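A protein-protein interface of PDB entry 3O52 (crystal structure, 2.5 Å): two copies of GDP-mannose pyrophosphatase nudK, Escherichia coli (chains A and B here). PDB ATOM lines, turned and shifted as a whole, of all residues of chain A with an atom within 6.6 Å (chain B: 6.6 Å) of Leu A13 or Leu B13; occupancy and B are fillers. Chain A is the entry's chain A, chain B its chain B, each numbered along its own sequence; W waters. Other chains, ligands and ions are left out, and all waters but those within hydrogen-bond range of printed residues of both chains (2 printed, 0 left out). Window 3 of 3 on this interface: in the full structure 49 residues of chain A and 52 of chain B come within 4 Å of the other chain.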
ATOM      1  N   LYS A  11     -13.735  18.607  19.082  1.00  0.00           N
ATOM      2  CA  LYS A  11     -12.770  19.304  19.921  1.00  0.00           C
ATOM      3  C   LYS A  11     -12.292  20.613  19.285  1.00  0.00           C
ATOM      4  O   LYS A  11     -11.748  20.617  18.166  1.00  0.00           O
ATOM      5  CB  LYS A  11     -11.578  18.398  20.231  1.00  0.00           C
ATOM      6  CG  LYS A  11     -10.535  19.032  21.130  1.00  0.00           C
ATOM      7  CD  LYS A  11     -10.657  18.552  22.569  1.00  0.00           C
ATOM      8  CE  LYS A  11     -10.191  19.624  23.564  1.00  0.00           C
ATOM      9  NZ  LYS A  11      -8.980  20.343  23.029  1.00  0.00           N
ATOM     10  N   ILE A  12     -12.498  21.715  20.003  1.00  0.00           N
ATOM     11  CA  ILE A  12     -12.100  23.026  19.537  1.00  0.00           C
ATOM     12  C   ILE A  12     -10.614  23.161  19.791  1.00  0.00           C
ATOM     13  O   ILE A  12     -10.178  23.014  20.925  1.00  0.00           O
ATOM     14  CB  ILE A  12     -12.836  24.154  20.296  1.00  0.00           C
ATOM     15  CG1 ILE A  12     -14.358  24.044  20.126  1.00  0.00           C
ATOM     16  CG2 ILE A  12     -12.325  25.532  19.847  1.00  0.00           C
ATOM     17  CD1 ILE A  12     -14.787  23.812  18.683  1.00  0.00           C
ATOM     18  N   LEU A  13      -9.828  23.430  18.748  1.00  0.00           N
ATOM     19  CA  LEU A  13      -8.385  23.589  18.948  1.00  0.00           C
ATOM     20  C   LEU A  13      -7.983  25.059  19.046  1.00  0.00           C
ATOM     21  O   LEU A  13      -6.925  25.383  19.573  1.00  0.00           O
ATOM     22  CB  LEU A  13      -7.621  22.916  17.814  1.00  0.00           C
ATOM     23  CG  LEU A  13      -7.780  21.405  17.677  1.00  0.00           C
ATOM     24  CD1 LEU A  13      -7.215  20.983  16.317  1.00  0.00           C
ATOM     25  CD2 LEU A  13      -7.094  20.697  18.865  1.00  0.00           C
ATOM     26  N   SER A  14      -8.834  25.925  18.494  1.00  0.00           N
ATOM     27  CA  SER A  14      -8.690  27.381  18.554  1.00  0.00           C
ATOM     28  C   SER A  14      -9.981  28.062  18.096  1.00  0.00           C
ATOM     29  O   SER A  14     -10.640  27.603  17.176  1.00  0.00           O
ATOM     30  CB  SER A  14      -7.520  27.861  17.690  1.00  0.00           C
ATOM     31  OG  SER A  14      -7.784  29.138  17.141  1.00  0.00           O
ATOM     32  N   ASP A  15     -10.294  29.179  18.726  1.00  0.00           N
ATOM     33  CA  ASP A  15     -11.495  29.934  18.480  1.00  0.00           C
ATOM     34  C   ASP A  15     -11.163  31.411  18.704  1.00  0.00           C
ATOM     35  O   ASP A  15     -11.841  32.116  19.447  1.00  0.00           O
ATOM     36  CB  ASP A  15     -12.571  29.508  19.490  1.00  0.00           C
ATOM     37  CG  ASP A  15     -13.869  30.267  19.304  1.00  0.00           C
ATOM     38  OD1 ASP A  15     -14.240  30.538  18.123  1.00  0.00           O
ATOM     39  OD2 ASP A  15     -14.487  30.617  20.345  1.00  0.00           O
ATOM     40  N   ASN A  16     -10.073  31.843  18.093  1.00  0.00           N
ATOM     41  CA  ASN A  16      -9.606  33.225  18.115  1.00  0.00           C
ATOM     42  C   ASN A  16     -10.598  34.154  17.392  1.00  0.00           C
ATOM     43  O   ASN A  16     -10.934  35.223  17.877  1.00  0.00           O
ATOM     44  CB  ASN A  16      -8.227  33.263  17.420  1.00  0.00           C
ATOM     45  CG  ASN A  16      -7.731  34.671  17.156  1.00  0.00           C
ATOM     46  OD1 ASN A  16      -7.141  35.325  18.044  1.00  0.00           O
ATOM     47  ND2 ASN A  16      -7.930  35.141  15.917  1.00  0.00           N
ATOM     48  N   THR A  19     -12.834  29.220  13.728  1.00  0.00           N
ATOM     49  CA  THR A  19     -12.751  28.085  14.649  1.00  0.00           C
ATOM     50  C   THR A  19     -12.107  26.867  14.000  1.00  0.00           C
ATOM     51  O   THR A  19     -12.506  26.424  12.915  1.00  0.00           O
ATOM     52  CB  THR A  19     -14.149  27.684  15.198  1.00  0.00           C
ATOM     53  OG1 THR A  19     -14.986  28.848  15.325  1.00  0.00           O
ATOM     54  CG2 THR A  19     -14.018  27.008  16.574  1.00  0.00           C
ATOM     55  N   LEU A  20     -11.087  26.331  14.658  1.00  0.00           N
ATOM     56  CA  LEU A  20     -10.444  25.100  14.187  1.00  0.00           C
ATOM     57  C   LEU A  20     -10.918  23.965  15.094  1.00  0.00           C
ATOM     58  O   LEU A  20     -10.924  24.099  16.341  1.00  0.00           O
ATOM     59  CB  LEU A  20      -8.924  25.230  14.229  1.00  0.00           C
ATOM     60  CG  LEU A  20      -8.107  24.071  13.652  1.00  0.00           C
ATOM     61  CD1 LEU A  20      -8.462  23.848  12.191  1.00  0.00           C
ATOM     62  CD2 LEU A  20      -6.629  24.338  13.801  1.00  0.00           C
ATOM     63  N   HIS A  21     -11.311  22.862  14.465  1.00  0.00           N
ATOM     64  CA  HIS A  21     -11.823  21.700  15.169  1.00  0.00           C
ATOM     65  C   HIS A  21     -10.949  20.469  14.899  1.00  0.00           C
ATOM     66  O   HIS A  21     -10.359  20.323  13.811  1.00  0.00           O
ATOM     67  CB  HIS A  21     -13.201  21.328  14.635  1.00  0.00           C
ATOM     68  CG  HIS A  21     -14.267  22.370  14.803  1.00  0.00           C
ATOM     69  ND1 HIS A  21     -14.354  23.484  13.999  1.00  0.00           N
ATOM     70  CD2 HIS A  21     -15.361  22.397  15.599  1.00  0.00           C
ATOM     71  CE1 HIS A  21     -15.432  24.178  14.326  1.00  0.00           C
ATOM     72  NE2 HIS A  21     -16.052  23.549  15.306  1.00  0.00           N
ATOM     73  N   ASN A  22     -10.893  19.569  15.871  1.00  0.00           N
ATOM     74  CA  ASN A  22     -10.460  18.211  15.609  1.00  0.00           C
ATOM     75  C   ASN A  22     -11.727  17.396  15.746  1.00  0.00           C
ATOM     76  O   ASN A  22     -12.280  17.321  16.831  1.00  0.00           O
ATOM     77  CB  ASN A  22      -9.426  17.758  16.639  1.00  0.00           C
ATOM     78  CG  ASN A  22      -8.302  16.894  16.038  1.00  0.00           C
ATOM     79  OD1 ASN A  22      -8.302  16.561  14.855  1.00  0.00           O
ATOM     80  ND2 ASN A  22      -7.332  16.544  16.866  1.00  0.00           N
ATOM     81  N   ARG A  39      -9.913  14.184  12.090  1.00  0.00           N
ATOM     82  CA  ARG A  39      -9.428  15.195  11.144  1.00  0.00           C
ATOM     83  C   ARG A  39      -9.526  16.617  11.707  1.00  0.00           C
ATOM     84  O   ARG A  39     -10.427  16.930  12.478  1.00  0.00           O
ATOM     85  CB  ARG A  39     -10.251  15.120   9.859  1.00  0.00           C
ATOM     86  CG  ARG A  39     -10.021  13.864   9.047  1.00  0.00           C
ATOM     87  CD  ARG A  39      -9.149  14.129   7.844  1.00  0.00           C
ATOM     88  NE  ARG A  39      -9.511  13.281   6.709  1.00  0.00           N
ATOM     89  CZ  ARG A  39      -9.544  11.941   6.711  1.00  0.00           C
ATOM     90  NH1 ARG A  39      -9.229  11.252   7.807  1.00  0.00           N
ATOM     91  NH2 ARG A  39      -9.905  11.283   5.602  1.00  0.00           N
ATOM     92  N   GLU A  40      -8.584  17.466  11.331  1.00  0.00           N
ATOM     93  CA  GLU A  40      -8.677  18.882  11.630  1.00  0.00           C
ATOM     94  C   GLU A  40      -9.667  19.419  10.650  1.00  0.00           C
ATOM     95  O   GLU A  40      -9.660  19.022   9.497  1.00  0.00           O
ATOM     96  CB  GLU A  40      -7.341  19.606  11.425  1.00  0.00           C
ATOM     97  CG  GLU A  40      -6.266  19.134  12.366  1.00  0.00           C
ATOM     98  CD  GLU A  40      -5.141  20.142  12.580  1.00  0.00           C
ATOM     99  OE1 GLU A  40      -5.273  21.313  12.139  1.00  0.00           O
ATOM    100  OE2 GLU A  40      -4.129  19.748  13.203  1.00  0.00           O
ATOM    101  N   VAL A  41     -10.523  20.318  11.115  1.00  0.00           N
ATOM    102  CA  VAL A  41     -11.447  21.010  10.243  1.00  0.00           C
ATOM    103  C   VAL A  41     -11.438  22.493  10.593  1.00  0.00           C
ATOM    104  O   VAL A  41     -11.673  22.874  11.762  1.00  0.00           O
ATOM    105  CB  VAL A  41     -12.875  20.468  10.392  1.00  0.00           C
ATOM    106  CG1 VAL A  41     -13.874  21.369   9.643  1.00  0.00           C
ATOM    107  CG2 VAL A  41     -12.959  18.991   9.932  1.00  0.00           C
ATOM    108  N   LYS B  11       2.308  33.899  16.242  1.00  0.00           N
ATOM    109  CA  LYS B  11       1.755  33.260  17.423  1.00  0.00           C
ATOM    110  C   LYS B  11       1.177  31.927  16.977  1.00  0.00           C
ATOM    111  O   LYS B  11       0.435  31.893  15.988  1.00  0.00           O
ATOM    112  CB  LYS B  11       0.674  34.173  18.029  1.00  0.00           C
ATOM    113  CG  LYS B  11      -0.217  33.580  19.145  1.00  0.00           C
ATOM    114  CD  LYS B  11       0.557  33.315  20.430  1.00  0.00           C
ATOM    115  CE  LYS B  11      -0.195  32.350  21.341  1.00  0.00           C
ATOM    116  NZ  LYS B  11       0.556  32.177  22.632  1.00  0.00           N
ATOM    117  N   ILE B  12       1.523  30.833  17.664  1.00  0.00           N
ATOM    118  CA  ILE B  12       0.950  29.538  17.299  1.00  0.00           C
ATOM    119  C   ILE B  12      -0.306  29.312  18.093  1.00  0.00           C
ATOM    120  O   ILE B  12      -0.255  29.136  19.310  1.00  0.00           O
ATOM    121  CB  ILE B  12       1.896  28.315  17.491  1.00  0.00           C
ATOM    122  CG1 ILE B  12       3.271  28.532  16.835  1.00  0.00           C
ATOM    123  CG2 ILE B  12       1.254  27.053  16.893  1.00  0.00           C
ATOM    124  CD1 ILE B  12       3.268  28.454  15.342  1.00  0.00           C
ATOM    125  N   LEU B  13      -1.435  29.318  17.392  1.00  0.00           N
ATOM    126  CA  LEU B  13      -2.729  29.020  17.995  1.00  0.00           C
ATOM    127  C   LEU B  13      -3.025  27.523  18.017  1.00  0.00           C
ATOM    128  O   LEU B  13      -3.762  27.072  18.873  1.00  0.00           O
ATOM    129  CB  LEU B  13      -3.833  29.733  17.238  1.00  0.00           C
ATOM    130  CG  LEU B  13      -3.583  31.212  16.975  1.00  0.00           C
ATOM    131  CD1 LEU B  13      -4.424  31.637  15.750  1.00  0.00           C
ATOM    132  CD2 LEU B  13      -3.874  32.047  18.223  1.00  0.00           C
ATOM    133  N   SER B  14      -2.482  26.763  17.058  1.00  0.00           N
ATOM    134  CA  SER B  14      -2.564  25.301  17.125  1.00  0.00           C
ATOM    135  C   SER B  14      -1.468  24.557  16.365  1.00  0.00           C
ATOM    136  O   SER B  14      -1.074  24.942  15.268  1.00  0.00           O
ATOM    137  CB  SER B  14      -3.949  24.799  16.696  1.00  0.00           C
ATOM    138  OG  SER B  14      -3.983  23.382  16.548  1.00  0.00           O
ATOM    139  N   ASP B  15      -1.003  23.477  16.979  1.00  0.00           N
ATOM    140  CA  ASP B  15       0.059  22.652  16.433  1.00  0.00           C
ATOM    141  C   ASP B  15      -0.307  21.167  16.574  1.00  0.00           C
ATOM    142  O   ASP B  15       0.563  20.296  16.752  1.00  0.00           O
ATOM    143  CB  ASP B  15       1.386  22.949  17.158  1.00  0.00           C
ATOM    144  CG  ASP B  15       2.614  22.570  16.313  1.00  0.00           C
ATOM    145  OD1 ASP B  15       2.480  21.763  15.342  1.00  0.00           O
ATOM    146  OD2 ASP B  15       3.721  23.094  16.614  1.00  0.00           O
ATOM    147  N   ASN B  16      -1.601  20.884  16.513  1.00  0.00           N
ATOM    148  CA  ASN B  16      -2.068  19.515  16.598  1.00  0.00           C
ATOM    149  C   ASN B  16      -1.486  18.600  15.509  1.00  0.00           C
ATOM    150  O   ASN B  16      -1.126  17.464  15.797  1.00  0.00           O
ATOM    151  CB  ASN B  16      -3.587  19.470  16.554  1.00  0.00           C
ATOM    152  CG  ASN B  16      -4.109  18.070  16.384  1.00  0.00           C
ATOM    153  OD1 ASN B  16      -4.093  17.278  17.336  1.00  0.00           O
ATOM    154  ND2 ASN B  16      -4.563  17.739  15.159  1.00  0.00           N
ATOM    155  N   TYR B  17      -1.429  19.086  14.267  1.00  0.00           N
ATOM    156  CA  TYR B  17      -0.861  18.333  13.171  1.00  0.00           C
ATOM    157  C   TYR B  17      -0.474  19.283  12.058  1.00  0.00           C
ATOM    158  O   TYR B  17       0.685  19.351  11.664  1.00  0.00           O
ATOM    159  CB  TYR B  17      -1.828  17.269  12.619  1.00  0.00           C
ATOM    160  CG  TYR B  17      -1.195  16.465  11.492  1.00  0.00           C
ATOM    161  CD1 TYR B  17      -0.404  15.350  11.762  1.00  0.00           C
ATOM    162  CD2 TYR B  17      -1.351  16.851  10.170  1.00  0.00           C
ATOM    163  CE1 TYR B  17       0.195  14.616  10.739  1.00  0.00           C
ATOM    164  CE2 TYR B  17      -0.751  16.126   9.124  1.00  0.00           C
ATOM    165  CZ  TYR B  17       0.016  15.006   9.419  1.00  0.00           C
ATOM    166  OH  TYR B  17       0.605  14.307   8.391  1.00  0.00           O
ATOM    167  N   THR B  19      -0.704  23.485  11.218  1.00  0.00           N
ATOM    168  CA  THR B  19      -0.385  24.593  12.103  1.00  0.00           C
ATOM    169  C   THR B  19      -1.218  25.828  11.801  1.00  0.00           C
ATOM    170  O   THR B  19      -1.236  26.317  10.659  1.00  0.00           O
ATOM    171  CB  THR B  19       1.084  24.950  12.011  1.00  0.00           C
ATOM    172  OG1 THR B  19       1.846  23.748  12.114  1.00  0.00           O
ATOM    173  CG2 THR B  19       1.493  25.857  13.135  1.00  0.00           C
ATOM    174  N   LEU B  20      -1.883  26.329  12.842  1.00  0.00           N
ATOM    175  CA  LEU B  20      -2.620  27.576  12.747  1.00  0.00           C
ATOM    176  C   LEU B  20      -1.826  28.701  13.381  1.00  0.00           C
ATOM    177  O   LEU B  20      -1.497  28.650  14.568  1.00  0.00           O
ATOM    178  CB  LEU B  20      -3.992  27.447  13.407  1.00  0.00           C
ATOM    179  CG  LEU B  20      -4.936  28.646  13.257  1.00  0.00           C
ATOM    180  CD1 LEU B  20      -5.268  29.001  11.790  1.00  0.00           C
ATOM    181  CD2 LEU B  20      -6.213  28.493  14.124  1.00  0.00           C
ATOM    182  N   HIS B  21      -1.509  29.711  12.577  1.00  0.00           N
ATOM    183  CA  HIS B  21      -0.784  30.877  13.086  1.00  0.00           C
ATOM    184  C   HIS B  21      -1.700  32.073  13.192  1.00  0.00           C
ATOM    185  O   HIS B  21      -2.735  32.164  12.510  1.00  0.00           O
ATOM    186  CB  HIS B  21       0.363  31.296  12.184  1.00  0.00           C
ATOM    187  CG  HIS B  21       1.355  30.217  11.886  1.00  0.00           C
ATOM    188  ND1 HIS B  21       1.084  29.171  11.032  1.00  0.00           N
ATOM    189  CD2 HIS B  21       2.641  30.061  12.271  1.00  0.00           C
ATOM    190  CE1 HIS B  21       2.157  28.409  10.918  1.00  0.00           C
ATOM    191  NE2 HIS B  21       3.111  28.921  11.672  1.00  0.00           N
ATOM    192  N   ASN B  22      -1.300  32.980  14.075  1.00  0.00           N
ATOM    193  CA  ASN B  22      -1.844  34.325  14.150  1.00  0.00           C
ATOM    194  C   ASN B  22      -0.640  35.174  13.831  1.00  0.00           C
ATOM    195  O   ASN B  22       0.360  35.144  14.541  1.00  0.00           O
ATOM    196  CB  ASN B  22      -2.383  34.636  15.552  1.00  0.00           C
ATOM    197  CG  ASN B  22      -3.502  35.674  15.537  1.00  0.00           C
ATOM    198  OD1 ASN B  22      -4.029  36.018  14.478  1.00  0.00           O
ATOM    199  ND2 ASN B  22      -3.860  36.178  16.710  1.00  0.00           N
ATOM    200  N   ILE B  23      -0.712  35.907  12.741  1.00  0.00           N
ATOM    201  CA  ILE B  23       0.457  36.596  12.250  1.00  0.00           C
ATOM    202  C   ILE B  23       0.237  38.094  12.308  1.00  0.00           C
ATOM    203  O   ILE B  23      -0.708  38.631  11.735  1.00  0.00           O
ATOM    204  CB  ILE B  23       0.821  36.083  10.841  1.00  0.00           C
ATOM    205  CG1 ILE B  23       1.470  34.700  10.986  1.00  0.00           C
ATOM    206  CG2 ILE B  23       1.783  37.029  10.133  1.00  0.00           C
ATOM    207  CD1 ILE B  23       1.647  33.967   9.720  1.00  0.00           C
ATOM    208  N   ARG B  39      -3.706  38.735  11.378  1.00  0.00           N
ATOM    209  CA  ARG B  39      -4.598  37.778  10.705  1.00  0.00           C
ATOM    210  C   ARG B  39      -4.279  36.315  10.988  1.00  0.00           C
ATOM    211  O   ARG B  39      -3.111  35.937  11.075  1.00  0.00           O
ATOM    212  CB  ARG B  39      -4.586  37.991   9.173  1.00  0.00           C
ATOM    213  CG  ARG B  39      -5.306  39.267   8.732  1.00  0.00           C
ATOM    214  CD  ARG B  39      -5.348  39.445   7.232  1.00  0.00           C
ATOM    215  NE  ARG B  39      -6.065  38.358   6.559  1.00  0.00           N
ATOM    216  CZ  ARG B  39      -7.389  38.278   6.448  1.00  0.00           C
ATOM    217  NH1 ARG B  39      -8.167  39.209   6.994  1.00  0.00           N
ATOM    218  NH2 ARG B  39      -7.938  37.253   5.802  1.00  0.00           N
ATOM    219  N   GLU B  40      -5.319  35.491  11.099  1.00  0.00           N
ATOM    220  CA  GLU B  40      -5.144  34.042  11.202  1.00  0.00           C
ATOM    221  C   GLU B  40      -4.627  33.454   9.884  1.00  0.00           C
ATOM    222  O   GLU B  40      -5.145  33.775   8.825  1.00  0.00           O
ATOM    223  CB  GLU B  40      -6.457  33.362  11.559  1.00  0.00           C
ATOM    224  CG  GLU B  40      -6.876  33.515  13.000  1.00  0.00           C
ATOM    225  CD  GLU B  40      -8.164  32.805  13.281  1.00  0.00           C
ATOM    226  OE1 GLU B  40      -8.400  31.780  12.619  1.00  0.00           O
ATOM    227  OE2 GLU B  40      -8.942  33.246  14.165  1.00  0.00           O
ATOM    228  N   VAL B  41      -3.601  32.606   9.957  1.00  0.00           N
ATOM    229  CA  VAL B  41      -3.098  31.893   8.792  1.00  0.00           C
ATOM    230  C   VAL B  41      -2.948  30.423   9.120  1.00  0.00           C
ATOM    231  O   VAL B  41      -2.204  30.069  10.047  1.00  0.00           O
ATOM    232  CB  VAL B  41      -1.711  32.398   8.375  1.00  0.00           C
ATOM    233  CG1 VAL B  41      -1.172  31.566   7.220  1.00  0.00           C
ATOM    234  CG2 VAL B  41      -1.776  33.860   7.999  1.00  0.00           C
HETATM  235  O   HOH W   1      -5.988  15.505  14.193  1.00  0.00           O
HETATM  236  O   HOH W   2      -3.423  22.645  14.165  1.00  0.00           O
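Leu A13 touches Ser B14, and with the chains exchanged Ser A14 touches Leu B13. Leu A13 touches Asn B16, but with the chains exchanged Asn A16 does not touch Leu B13 (4.5 Å). Ser A14 touches Leu B20, and with the chains exchanged Leu A20 touches Ser B14. Asn A16 touches Glu B40, and with the chains exchanged Glu A40 touches Asn B16. Of the 11 pairs that touch across the chains among the printed residues, 9 have their exchanged pair printed and touching as well.
Printed residues of chain B that touch a printed residue of chain A: Leu B13, Ser B14, Asn B16, Tyr B17, Leu B20, Asn B22 and Glu B40. Hydrophobic or aromatic side chains of chain B that line the printed part of chain A: Leu B13, Tyr B17 and Leu B20. Hydrophobic or aromatic side chains of chain A within 4 Å of the printed part of chain B: Leu A13 and Leu A20. Among the printed residues, 11 pairs touch across the chains.
Water W2 lies within hydrogen-bond range of OG of Ser B14, OE1 of Glu A40 and N of Asn B16. Water W1 lies within hydrogen-bond range of the side-chain amide oxygen (OD1) of Asn A22 and the side-chain amide nitrogen (ND2) of Asn B16.
The side-chain amide nitrogen of Asn A22 is in hydrogen-bond range of the side-chain amide oxygen of Asn B16. The side-chain amide nitrogen (ND2) of Asn A16 sits at hydrogen-bond distance from the side-chain carboxylate (OE2) of Glu B40 (2.8 Å). OE2 of Glu A40 sits at hydrogen-bond distance from ND2 of Asn B16 (2.8 Å). The side-chain carboxylate of Glu A40 is in hydrogen-bond range of the backbone NH of Tyr B17.
Leu A13 touches Leu B13 (O to O, 3.7 Å). Leu A13 touches Ser B14. Leu A13 touches Asn B16 (CD1 to CB, 3.9 Å). Leu B13 touches Ser A14 (CB to OG, 3.997 Å). Ser A14 touches Leu B20 (OG to CD2, 3.5 Å). Asn A16 touches Asn B22 (OD1 to ND2, 3.6 Å). Ser B14 touches Leu A20 (OG to CD2, 3.9 Å).
The backbone carbonyl oxygen of Lys B11 sits at hydrogen-bond distance from the backbone NH of Asn B22 (2.8 Å). O of Ser B14 lies within hydrogen-bond range of N of Leu B20. The side-chain hydroxyl (OG) of Ser B14 lies within hydrogen-bond range of the backbone NH (N) of Asn B16, at 3.5 Å. The backbone NH (N) of Leu A13 sits at hydrogen-bond distance from the backbone carbonyl oxygen (O) of Leu A20 (2.7 Å). The backbone NH (N) of Leu B13 sits at hydrogen-bond distance from the backbone carbonyl oxygen (O) of Leu B20 (2.9 Å). The backbone carbonyl oxygen of Lys A11 is in hydrogen-bond range of the backbone NH of Asn A22 (2.7 Å).
Of the printed residues of chain A, Leu B13 touches Leu A13 (3.7 Å) and Ser A14 (3.997 Å). Of the printed residues of chain B, Leu A20 touches Ser B14. Printed residues of chain B within 4 Å of Asn A22: Asn B16. Of the printed residues of chain B, Asn A16 touches Asn B22 and Glu B40. Arg B39 touches none of the printed residues of chain A. Lys A11 touches none of the printed residues of chain B. The nearest residue of chain B that does not touch Leu A13 is Leu B20 (6.3 Å). The nearest printed residue of chain A that does not touch Leu B13 is Asn A16 (4.5 Å).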
